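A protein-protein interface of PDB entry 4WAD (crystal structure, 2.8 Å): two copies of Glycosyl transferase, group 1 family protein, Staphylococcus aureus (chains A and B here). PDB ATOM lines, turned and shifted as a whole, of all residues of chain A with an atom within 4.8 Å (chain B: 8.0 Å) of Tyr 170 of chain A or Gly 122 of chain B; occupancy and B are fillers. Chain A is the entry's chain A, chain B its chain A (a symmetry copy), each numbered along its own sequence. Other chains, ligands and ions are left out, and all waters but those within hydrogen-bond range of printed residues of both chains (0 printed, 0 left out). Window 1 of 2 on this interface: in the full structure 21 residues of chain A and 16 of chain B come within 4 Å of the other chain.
Of the printed residues of chain B, Tyr 170 of chain A touches Phe 117, Gly 122, Tyr 124 and Asn 143. Of chain A, only Tyr 170, Val 172 and Pro 180 come within 4 Å of Gly 122 of chain B. Cys 169 of chain A touches three residues of chain B. Of the printed residues of chain A, Thr 120 of chain B touches Tyr 174 and Pro 180. Of the printed residues of chain A, Lys 144 of chain B touches Cys 169. Of the printed residues of chain A, Asp 142 of chain B touches Thr 161 (3.8 Å) and Cys 169 (3.9 Å). Printed residues of chain B within 4 Å of Leu 199 of chain A: Phe 117. Printed residues of chain B within 4 Å of Thr 161 of chain A: Asp 142. The nearest printed residue of chain A that does not touch Gly 122 of chain B is Ser 183 of chain A (4.1 Å). The nearest printed residue of chain A that does not touch Phe 117 of chain B is Asn 185 of chain A (6.4 Å).
The backbone carbonyl oxygen of Thr 161 of chain A sits at hydrogen-bond distance from the backbone NH of Cys 169 of chain A (3.0 Å). N of Thr 161 of chain A is in hydrogen-bond range of O of Tyr 170 of chain A, at 3.0 Å. N of Ile 186 of chain A lies within hydrogen-bond range of O of Cys 169 of chain A. OG of Ser 183 of chain A lies within hydrogen-bond range of OH of Tyr 170 of chain A, at 2.7 Å. O of Asn 103 of chain B sits at hydrogen-bond distance from N of Ile 119 of chain B (3.0 Å). The backbone NH (N) of Thr 121 of chain B is in hydrogen-bond range of the side-chain carboxylate (OD2) of Asp 118 of chain B, 2.5 Å away.
No position is printed for both chains. Of the 19 pairs that touch across the chains among the printed residues, none has its exchanged pair printed and touching as well.
ND2 of Asn 143 of chain B sits at hydrogen-bond distance from O of Cys 169 of chain A, at 3.3 Å. SG of Cys 169 of chain A sits at hydrogen-bond distance from NZ of Lys 144 of chain B (3.7 Å). O of Gly 122 of chain B is in hydrogen-bond range of OH of Tyr 170 of chain A (3.0 Å). OD1 of Asn 185 of chain A lies within hydrogen-bond range of ND2 of Asn 143 of chain B (3.1 Å). O of Thr 121 of chain B sits close to OH of Tyr 174 of chain A (2.3 Å).
Printed residues of chain A that touch a printed residue of chain B: Lys 159, Thr 161, Cys 169, Tyr 170, Val 172, Tyr 174, Pro 180, Ser 183, Asn 185 and Leu 199. Hydrophobic or aromatic side chains of chain A that line the printed part of chain B: Tyr 170, Val 172, Tyr 174, Pro 180 and Leu 199. Along chain A the printed residues that touch a printed residue of chain B span positions 159 to 199. Printed residues of chain B that touch a printed residue of chain A: Phe 117, Ile 119, Thr 120, Thr 121, Gly 122, Thr 123, Tyr 124, Asp 142, Asn 143 and Lys 144. Among the printed residues, 19 pairs touch across the chains.
O of Asp 142 of chain B touches SG of Cys 169 of chain A, 3.9 Å away. N of Tyr 124 of chain B touches OH of Tyr 170 of chain A (3.8 Å). OD1 of Asn 143 of chain B touches CD1 of Tyr 170 of chain A, 3.4 Å away. O of Gly 122 of chain B touches CG2 of Val 172 of chain A, 3.8 Å away. O of Thr 120 of chain B touches CE2 of Tyr 174 of chain A, 3.8 Å away. Pro 180 of chain A touches Ile 119 of chain B. Thr 120 of chain B touches Pro 180 of chain A. Pro 180 of chain A touches Gly 122 of chain B. Phe 117 of chain B touches Ser 183 of chain A (CE2 to OG, 3.96 Å). Leu 199 of chain A touches Phe 117 of chain B (CD2 to CG, 3.7 Å).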
ATOM      1  N   LYS A 159      23.618  19.709  -9.870  1.00  0.00           N
ATOM      2  CA  LYS A 159      22.251  19.532 -10.344  1.00  0.00           C
ATOM      3  C   LYS A 159      22.090  18.115 -10.872  1.00  0.00           C
ATOM      4  O   LYS A 159      22.869  17.676 -11.720  1.00  0.00           O
ATOM      5  CB  LYS A 159      21.901  20.548 -11.437  1.00  0.00           C
ATOM      6  CG  LYS A 159      20.462  20.437 -11.937  1.00  0.00           C
ATOM      7  CD  LYS A 159      20.221  21.342 -13.134  1.00  0.00           C
ATOM      8  CE  LYS A 159      20.730  20.718 -14.425  1.00  0.00           C
ATOM      9  NZ  LYS A 159      19.953  19.504 -14.804  1.00  0.00           N
ATOM     10  N   GLU A 160      21.089  17.398 -10.370  1.00  0.00           N
ATOM     11  CA  GLU A 160      20.833  16.039 -10.832  1.00  0.00           C
ATOM     12  C   GLU A 160      19.547  15.980 -11.643  1.00  0.00           C
ATOM     13  O   GLU A 160      18.604  16.728 -11.379  1.00  0.00           O
ATOM     14  CB  GLU A 160      20.772  15.068  -9.644  1.00  0.00           C
ATOM     15  CG  GLU A 160      22.115  14.845  -8.968  1.00  0.00           C
ATOM     16  CD  GLU A 160      22.032  13.908  -7.779  1.00  0.00           C
ATOM     17  OE1 GLU A 160      21.294  14.224  -6.824  1.00  0.00           O
ATOM     18  OE2 GLU A 160      22.709  12.860  -7.800  1.00  0.00           O
ATOM     19  N   THR A 161      19.522  15.094 -12.635  1.00  0.00           N
ATOM     20  CA  THR A 161      18.360  14.933 -13.504  1.00  0.00           C
ATOM     21  C   THR A 161      17.807  13.518 -13.367  1.00  0.00           C
ATOM     22  O   THR A 161      18.575  12.560 -13.245  1.00  0.00           O
ATOM     23  CB  THR A 161      18.716  15.215 -14.972  1.00  0.00           C
ATOM     24  OG1 THR A 161      19.368  16.490 -15.069  1.00  0.00           O
ATOM     25  CG2 THR A 161      17.467  15.222 -15.835  1.00  0.00           C
ATOM     26  N   VAL A 168      18.724   8.873 -11.373  1.00  0.00           N
ATOM     27  CA  VAL A 168      19.652   9.838 -11.957  1.00  0.00           C
ATOM     28  C   VAL A 168      20.201   9.356 -13.300  1.00  0.00           C
ATOM     29  O   VAL A 168      20.636   8.209 -13.428  1.00  0.00           O
ATOM     30  CB  VAL A 168      20.826  10.135 -11.000  1.00  0.00           C
ATOM     31  CG1 VAL A 168      21.722  11.223 -11.568  1.00  0.00           C
ATOM     32  CG2 VAL A 168      20.295  10.558  -9.651  1.00  0.00           C
ATOM     33  N   CYS A 169      20.167  10.238 -14.297  1.00  0.00           N
ATOM     34  CA  CYS A 169      20.672   9.930 -15.630  1.00  0.00           C
ATOM     35  C   CYS A 169      21.612  11.022 -16.128  1.00  0.00           C
ATOM     36  O   CYS A 169      22.151  10.936 -17.233  1.00  0.00           O
ATOM     37  CB  CYS A 169      19.510   9.752 -16.613  1.00  0.00           C
ATOM     38  SG  CYS A 169      18.526  11.248 -16.865  1.00  0.00           S
ATOM     39  N   TYR A 170      21.797  12.053 -15.307  1.00  0.00           N
ATOM     40  CA  TYR A 170      22.633  13.190 -15.680  1.00  0.00           C
ATOM     41  C   TYR A 170      23.041  13.997 -14.456  1.00  0.00           C
ATOM     42  O   TYR A 170      22.233  14.216 -13.552  1.00  0.00           O
ATOM     43  CB  TYR A 170      21.890  14.083 -16.676  1.00  0.00           C
ATOM     44  CG  TYR A 170      22.746  15.095 -17.400  1.00  0.00           C
ATOM     45  CD1 TYR A 170      23.766  14.691 -18.246  1.00  0.00           C
ATOM     46  CD2 TYR A 170      22.497  16.453 -17.279  1.00  0.00           C
ATOM     47  CE1 TYR A 170      24.533  15.610 -18.930  1.00  0.00           C
ATOM     48  CE2 TYR A 170      23.256  17.384 -17.959  1.00  0.00           C
ATOM     49  CZ  TYR A 170      24.274  16.955 -18.783  1.00  0.00           C
ATOM     50  OH  TYR A 170      25.033  17.875 -19.466  1.00  0.00           O
ATOM     51  N   GLN A 171      24.297  14.435 -14.432  1.00  0.00           N
ATOM     52  CA  GLN A 171      24.804  15.264 -13.346  1.00  0.00           C
ATOM     53  C   GLN A 171      25.496  16.498 -13.903  1.00  0.00           C
ATOM     54  O   GLN A 171      26.044  16.460 -15.004  1.00  0.00           O
ATOM     55  CB  GLN A 171      25.771  14.468 -12.461  1.00  0.00           C
ATOM     56  CG  GLN A 171      25.098  13.422 -11.585  1.00  0.00           C
ATOM     57  CD  GLN A 171      26.092  12.620 -10.768  1.00  0.00           C
ATOM     58  OE1 GLN A 171      27.237  12.426 -11.174  1.00  0.00           O
ATOM     59  NE2 GLN A 171      25.656  12.149  -9.607  1.00  0.00           N
ATOM     60  N   VAL A 172      25.459  17.591 -13.148  1.00  0.00           N
ATOM     61  CA  VAL A 172      26.174  18.810 -13.511  1.00  0.00           C
ATOM     62  C   VAL A 172      26.865  19.332 -12.262  1.00  0.00           C
ATOM     63  O   VAL A 172      26.284  19.294 -11.179  1.00  0.00           O
ATOM     64  CB  VAL A 172      25.235  19.892 -14.086  1.00  0.00           C
ATOM     65  CG1 VAL A 172      26.021  21.142 -14.450  1.00  0.00           C
ATOM     66  CG2 VAL A 172      24.505  19.373 -15.300  1.00  0.00           C
ATOM     67  N   TYR A 174      28.811  22.615 -10.454  1.00  0.00           N
ATOM     68  CA  TYR A 174      29.002  24.058 -10.536  1.00  0.00           C
ATOM     69  C   TYR A 174      30.176  24.485  -9.659  1.00  0.00           C
ATOM     70  O   TYR A 174      30.365  23.940  -8.564  1.00  0.00           O
ATOM     71  CB  TYR A 174      27.718  24.793 -10.127  1.00  0.00           C
ATOM     72  CG  TYR A 174      26.503  24.384 -10.933  1.00  0.00           C
ATOM     73  CD1 TYR A 174      25.739  23.284 -10.565  1.00  0.00           C
ATOM     74  CD2 TYR A 174      26.123  25.094 -12.063  1.00  0.00           C
ATOM     75  CE1 TYR A 174      24.633  22.903 -11.298  1.00  0.00           C
ATOM     76  CE2 TYR A 174      25.016  24.719 -12.803  1.00  0.00           C
ATOM     77  CZ  TYR A 174      24.277  23.623 -12.414  1.00  0.00           C
ATOM     78  OH  TYR A 174      23.177  23.248 -13.148  1.00  0.00           O
ATOM     79  N   PRO A 180      28.745  26.009 -14.329  1.00  0.00           N
ATOM     80  CA  PRO A 180      28.960  24.589 -14.624  1.00  0.00           C
ATOM     81  C   PRO A 180      30.308  24.355 -15.301  1.00  0.00           C
ATOM     82  O   PRO A 180      30.628  25.044 -16.275  1.00  0.00           O
ATOM     83  CB  PRO A 180      27.801  24.247 -15.571  1.00  0.00           C
ATOM     84  CG  PRO A 180      27.460  25.551 -16.229  1.00  0.00           C
ATOM     85  CD  PRO A 180      27.689  26.599 -15.174  1.00  0.00           C
ATOM     86  N   SER A 183      29.736  18.146 -16.740  1.00  0.00           N
ATOM     87  CA  SER A 183      28.477  17.410 -16.755  1.00  0.00           C
ATOM     88  C   SER A 183      28.732  16.017 -17.309  1.00  0.00           C
ATOM     89  O   SER A 183      29.680  15.824 -18.073  1.00  0.00           O
ATOM     90  CB  SER A 183      27.429  18.132 -17.589  1.00  0.00           C
ATOM     91  OG  SER A 183      27.676  17.955 -18.968  1.00  0.00           O
ATOM     92  N   ARG A 184      27.897  15.049 -16.933  1.00  0.00           N
ATOM     93  CA  ARG A 184      28.124  13.668 -17.359  1.00  0.00           C
ATOM     94  C   ARG A 184      26.856  12.819 -17.350  1.00  0.00           C
ATOM     95  O   ARG A 184      25.945  13.048 -16.551  1.00  0.00           O
ATOM     96  CB  ARG A 184      29.189  13.013 -16.473  1.00  0.00           C
ATOM     97  CG  ARG A 184      28.815  12.932 -15.001  1.00  0.00           C
ATOM     98  CD  ARG A 184      29.942  12.316 -14.191  1.00  0.00           C
ATOM     99  NE  ARG A 184      29.564  12.052 -12.805  1.00  0.00           N
ATOM    100  CZ  ARG A 184      30.333  11.421 -11.926  1.00  0.00           C
ATOM    101  NH1 ARG A 184      31.527  10.985 -12.285  1.00  0.00           N
ATOM    102  NH2 ARG A 184      29.904  11.224 -10.687  1.00  0.00           N
ATOM    103  N   ASN A 185      26.808  11.839 -18.246  1.00  0.00           N
ATOM    104  CA  ASN A 185      25.678  10.923 -18.317  1.00  0.00           C
ATOM    105  C   ASN A 185      25.823   9.787 -17.310  1.00  0.00           C
ATOM    106  O   ASN A 185      26.932   9.310 -17.062  1.00  0.00           O
ATOM    107  CB  ASN A 185      25.537  10.359 -19.734  1.00  0.00           C
ATOM    108  CG  ASN A 185      25.256  11.432 -20.761  1.00  0.00           C
ATOM    109  OD1 ASN A 185      24.665  12.466 -20.451  1.00  0.00           O
ATOM    110  ND2 ASN A 185      25.688  11.197 -21.997  1.00  0.00           N
ATOM    111  N   ILE A 186      24.701   9.365 -16.734  1.00  0.00           N
ATOM    112  CA  ILE A 186      24.690   8.264 -15.776  1.00  0.00           C
ATOM    113  C   ILE A 186      23.746   7.168 -16.257  1.00  0.00           C
ATOM    114  O   ILE A 186      22.589   7.442 -16.575  1.00  0.00           O
ATOM    115  CB  ILE A 186      24.253   8.732 -14.365  1.00  0.00           C
ATOM    116  CG1 ILE A 186      25.209   9.796 -13.823  1.00  0.00           C
ATOM    117  CG2 ILE A 186      24.164   7.545 -13.402  1.00  0.00           C
ATOM    118  CD1 ILE A 186      26.609   9.281 -13.562  1.00  0.00           C
ATOM    119  N   LEU A 199      32.941  21.136 -19.628  1.00  0.00           N
ATOM    120  CA  LEU A 199      32.373  22.345 -20.218  1.00  0.00           C
ATOM    121  C   LEU A 199      33.347  23.525 -20.207  1.00  0.00           C
ATOM    122  O   LEU A 199      33.336  24.357 -21.118  1.00  0.00           O
ATOM    123  CB  LEU A 199      31.084  22.723 -19.478  1.00  0.00           C
ATOM    124  CG  LEU A 199      30.024  21.626 -19.333  1.00  0.00           C
ATOM    125  CD1 LEU A 199      28.892  22.047 -18.408  1.00  0.00           C
ATOM    126  CD2 LEU A 199      29.472  21.231 -20.687  1.00  0.00           C
ATOM    127  N   ASN B 103      22.698  30.901 -25.757  1.00  0.00           N
ATOM    128  CA  ASN B 103      23.223  30.724 -24.402  1.00  0.00           C
ATOM    129  C   ASN B 103      23.723  29.291 -24.195  1.00  0.00           C
ATOM    130  O   ASN B 103      23.634  28.740 -23.098  1.00  0.00           O
ATOM    131  CB  ASN B 103      22.165  31.088 -23.351  1.00  0.00           C
ATOM    132  CG  ASN B 103      22.752  31.269 -21.956  1.00  0.00           C
ATOM    133  OD1 ASN B 103      23.399  32.276 -21.666  1.00  0.00           O
ATOM    134  ND2 ASN B 103      22.518  30.294 -21.082  1.00  0.00           N
ATOM    135  N   ILE B 105      27.041  26.354 -25.041  1.00  0.00           N
ATOM    136  CA  ILE B 105      28.448  26.203 -25.390  1.00  0.00           C
ATOM    137  C   ILE B 105      28.603  24.974 -26.287  1.00  0.00           C
ATOM    138  O   ILE B 105      27.823  24.026 -26.189  1.00  0.00           O
ATOM    139  CB  ILE B 105      29.342  26.086 -24.130  1.00  0.00           C
ATOM    140  CG1 ILE B 105      30.721  26.692 -24.391  1.00  0.00           C
ATOM    141  CG2 ILE B 105      29.454  24.644 -23.646  1.00  0.00           C
ATOM    142  CD1 ILE B 105      30.668  28.162 -24.718  1.00  0.00           C
ATOM    143  N   TYR B 116      25.637  20.675 -27.622  1.00  0.00           N
ATOM    144  CA  TYR B 116      25.512  22.019 -27.076  1.00  0.00           C
ATOM    145  C   TYR B 116      24.943  21.985 -25.662  1.00  0.00           C
ATOM    146  O   TYR B 116      23.968  21.280 -25.393  1.00  0.00           O
ATOM    147  CB  TYR B 116      24.644  22.883 -27.997  1.00  0.00           C
ATOM    148  CG  TYR B 116      25.265  23.126 -29.357  1.00  0.00           C
ATOM    149  CD1 TYR B 116      25.200  22.162 -30.354  1.00  0.00           C
ATOM    150  CD2 TYR B 116      25.917  24.317 -29.640  1.00  0.00           C
ATOM    151  CE1 TYR B 116      25.767  22.376 -31.594  1.00  0.00           C
ATOM    152  CE2 TYR B 116      26.486  24.542 -30.880  1.00  0.00           C
ATOM    153  CZ  TYR B 116      26.407  23.568 -31.851  1.00  0.00           C
ATOM    154  OH  TYR B 116      26.970  23.783 -33.087  1.00  0.00           O
ATOM    155  N   PHE B 117      25.561  22.744 -24.763  1.00  0.00           N
ATOM    156  CA  PHE B 117      25.165  22.747 -23.359  1.00  0.00           C
ATOM    157  C   PHE B 117      24.904  24.167 -22.882  1.00  0.00           C
ATOM    158  O   PHE B 117      25.680  25.074 -23.180  1.00  0.00           O
ATOM    159  CB  PHE B 117      26.246  22.089 -22.494  1.00  0.00           C
ATOM    160  CG  PHE B 117      26.526  20.661 -22.854  1.00  0.00           C
ATOM    161  CD1 PHE B 117      27.485  20.344 -23.808  1.00  0.00           C
ATOM    162  CD2 PHE B 117      25.824  19.635 -22.242  1.00  0.00           C
ATOM    163  CE1 PHE B 117      27.740  19.023 -24.144  1.00  0.00           C
ATOM    164  CE2 PHE B 117      26.070  18.312 -22.572  1.00  0.00           C
ATOM    165  CZ  PHE B 117      27.030  18.007 -23.523  1.00  0.00           C
ATOM    166  N   ASP B 118      23.810  24.352 -22.147  1.00  0.00           N
ATOM    167  CA  ASP B 118      23.460  25.654 -21.596  1.00  0.00           C
ATOM    168  C   ASP B 118      24.552  26.138 -20.645  1.00  0.00           C
ATOM    169  O   ASP B 118      24.928  25.432 -19.709  1.00  0.00           O
ATOM    170  CB  ASP B 118      22.107  25.584 -20.883  1.00  0.00           C
ATOM    171  CG  ASP B 118      21.768  26.865 -20.140  1.00  0.00           C
ATOM    172  OD1 ASP B 118      21.333  27.840 -20.791  1.00  0.00           O
ATOM    173  OD2 ASP B 118      21.924  26.894 -18.903  1.00  0.00           O
ATOM    174  N   ILE B 119      25.060  27.343 -20.892  1.00  0.00           N
ATOM    175  CA  ILE B 119      26.180  27.881 -20.124  1.00  0.00           C
ATOM    176  C   ILE B 119      25.762  28.413 -18.756  1.00  0.00           C
ATOM    177  O   ILE B 119      26.595  28.922 -18.000  1.00  0.00           O
ATOM    178  CB  ILE B 119      26.889  29.005 -20.900  1.00  0.00           C
ATOM    179  CG1 ILE B 119      25.920  30.143 -21.197  1.00  0.00           C
ATOM    180  CG2 ILE B 119      27.477  28.477 -22.194  1.00  0.00           C
ATOM    181  CD1 ILE B 119      26.534  31.273 -22.009  1.00  0.00           C
ATOM    182  N   THR B 120      24.473  28.309 -18.443  1.00  0.00           N
ATOM    183  CA  THR B 120      23.967  28.759 -17.148  1.00  0.00           C
ATOM    184  C   THR B 120      23.689  27.571 -16.225  1.00  0.00           C
ATOM    185  O   THR B 120      24.022  27.600 -15.040  1.00  0.00           O
ATOM    186  CB  THR B 120      22.677  29.600 -17.301  1.00  0.00           C
ATOM    187  OG1 THR B 120      22.962  30.791 -18.046  1.00  0.00           O
ATOM    188  CG2 THR B 120      22.124  29.989 -15.938  1.00  0.00           C
ATOM    189  N   THR B 121      23.094  26.519 -16.783  1.00  0.00           N
ATOM    190  CA  THR B 121      22.695  25.356 -15.995  1.00  0.00           C
ATOM    191  C   THR B 121      23.561  24.131 -16.273  1.00  0.00           C
ATOM    192  O   THR B 121      23.667  23.241 -15.430  1.00  0.00           O
ATOM    193  CB  THR B 121      21.220  24.992 -16.247  1.00  0.00           C
ATOM    194  OG1 THR B 121      21.024  24.709 -17.638  1.00  0.00           O
ATOM    195  CG2 THR B 121      20.321  26.140 -15.832  1.00  0.00           C
ATOM    196  N   GLY B 122      24.167  24.083 -17.455  1.00  0.00           N
ATOM    197  CA  GLY B 122      24.956  22.930 -17.848  1.00  0.00           C
ATOM    198  C   GLY B 122      24.105  21.861 -18.504  1.00  0.00           C
ATOM    199  O   GLY B 122      24.579  20.760 -18.792  1.00  0.00           O
ATOM    200  N   THR B 123      22.840  22.195 -18.744  1.00  0.00           N
ATOM    201  CA  THR B 123      21.871  21.256 -19.307  1.00  0.00           C
ATOM    202  C   THR B 123      22.223  20.863 -20.743  1.00  0.00           C
ATOM    203  O   THR B 123      22.621  21.707 -21.549  1.00  0.00           O
ATOM    204  CB  THR B 123      20.446  21.847 -19.284  1.00  0.00           C
ATOM    205  OG1 THR B 123      20.101  22.217 -17.944  1.00  0.00           O
ATOM    206  CG2 THR B 123      19.440  20.832 -19.800  1.00  0.00           C
ATOM    207  N   TYR B 124      22.080  19.575 -21.050  1.00  0.00           N
ATOM    208  CA  TYR B 124      22.240  19.055 -22.406  1.00  0.00           C
ATOM    209  C   TYR B 124      21.124  19.585 -23.302  1.00  0.00           C
ATOM    210  O   TYR B 124      19.958  19.224 -23.128  1.00  0.00           O
ATOM    211  CB  TYR B 124      22.233  17.524 -22.386  1.00  0.00           C
ATOM    212  CG  TYR B 124      22.555  16.858 -23.708  1.00  0.00           C
ATOM    213  CD1 TYR B 124      23.197  17.548 -24.730  1.00  0.00           C
ATOM    214  CD2 TYR B 124      22.217  15.532 -23.927  1.00  0.00           C
ATOM    215  CE1 TYR B 124      23.489  16.932 -25.928  1.00  0.00           C
ATOM    216  CE2 TYR B 124      22.504  14.910 -25.121  1.00  0.00           C
ATOM    217  CZ  TYR B 124      23.142  15.617 -26.117  1.00  0.00           C
ATOM    218  OH  TYR B 124      23.435  15.006 -27.314  1.00  0.00           O
ATOM    219  N   ILE B 125      21.482  20.431 -24.263  1.00  0.00           N
ATOM    220  CA  ILE B 125      20.488  21.105 -25.090  1.00  0.00           C
ATOM    221  C   ILE B 125      20.283  20.456 -26.464  1.00  0.00           C
ATOM    222  O   ILE B 125      19.158  20.099 -26.825  1.00  0.00           O
ATOM    223  CB  ILE B 125      20.856  22.584 -25.306  1.00  0.00           C
ATOM    224  CG1 ILE B 125      20.797  23.349 -23.979  1.00  0.00           C
ATOM    225  CG2 ILE B 125      19.938  23.207 -26.341  1.00  0.00           C
ATOM    226  CD1 ILE B 125      19.480  23.184 -23.239  1.00  0.00           C
ATOM    227  N   ASP B 142      15.320  16.710 -20.228  1.00  0.00           N
ATOM    228  CA  ASP B 142      15.698  15.828 -19.125  1.00  0.00           C
ATOM    229  C   ASP B 142      16.661  14.752 -19.622  1.00  0.00           C
ATOM    230  O   ASP B 142      16.527  13.572 -19.287  1.00  0.00           O
ATOM    231  CB  ASP B 142      14.457  15.202 -18.481  1.00  0.00           C
ATOM    232  CG  ASP B 142      13.429  16.240 -18.068  1.00  0.00           C
ATOM    233  OD1 ASP B 142      13.828  17.384 -17.764  1.00  0.00           O
ATOM    234  OD2 ASP B 142      12.224  15.913 -18.062  1.00  0.00           O
ATOM    235  N   ASN B 143      17.620  15.190 -20.438  1.00  0.00           N
ATOM    236  CA  ASN B 143      18.670  14.342 -21.010  1.00  0.00           C
ATOM    237  C   ASN B 143      18.141  13.191 -21.873  1.00  0.00           C
ATOM    238  O   ASN B 143      18.856  12.222 -22.129  1.00  0.00           O
ATOM    239  CB  ASN B 143      19.569  13.780 -19.903  1.00  0.00           C
ATOM    240  CG  ASN B 143      21.013  13.634 -20.342  1.00  0.00           C
ATOM    241  OD1 ASN B 143      21.596  14.556 -20.910  1.00  0.00           O
ATOM    242  ND2 ASN B 143      21.595  12.465 -20.090  1.00  0.00           N
ATOM    243  N   LYS B 144      16.892  13.301 -22.321  1.00  0.00           N
ATOM    244  CA  LYS B 144      16.329  12.367 -23.296  1.00  0.00           C
ATOM    245  C   LYS B 144      15.973  13.124 -24.569  1.00  0.00           C
ATOM    246  O   LYS B 144      15.583  14.291 -24.501  1.00  0.00           O
ATOM    247  CB  LYS B 144      15.091  11.660 -22.733  1.00  0.00           C
ATOM    248  CG  LYS B 144      15.358  10.779 -21.528  1.00  0.00           C
ATOM    249  CD  LYS B 144      16.196   9.573 -21.910  1.00  0.00           C
ATOM    250  CE  LYS B 144      16.328   8.599 -20.752  1.00  0.00           C
ATOM    251  NZ  LYS B 144      16.996   9.214 -19.575  1.00  0.00           N
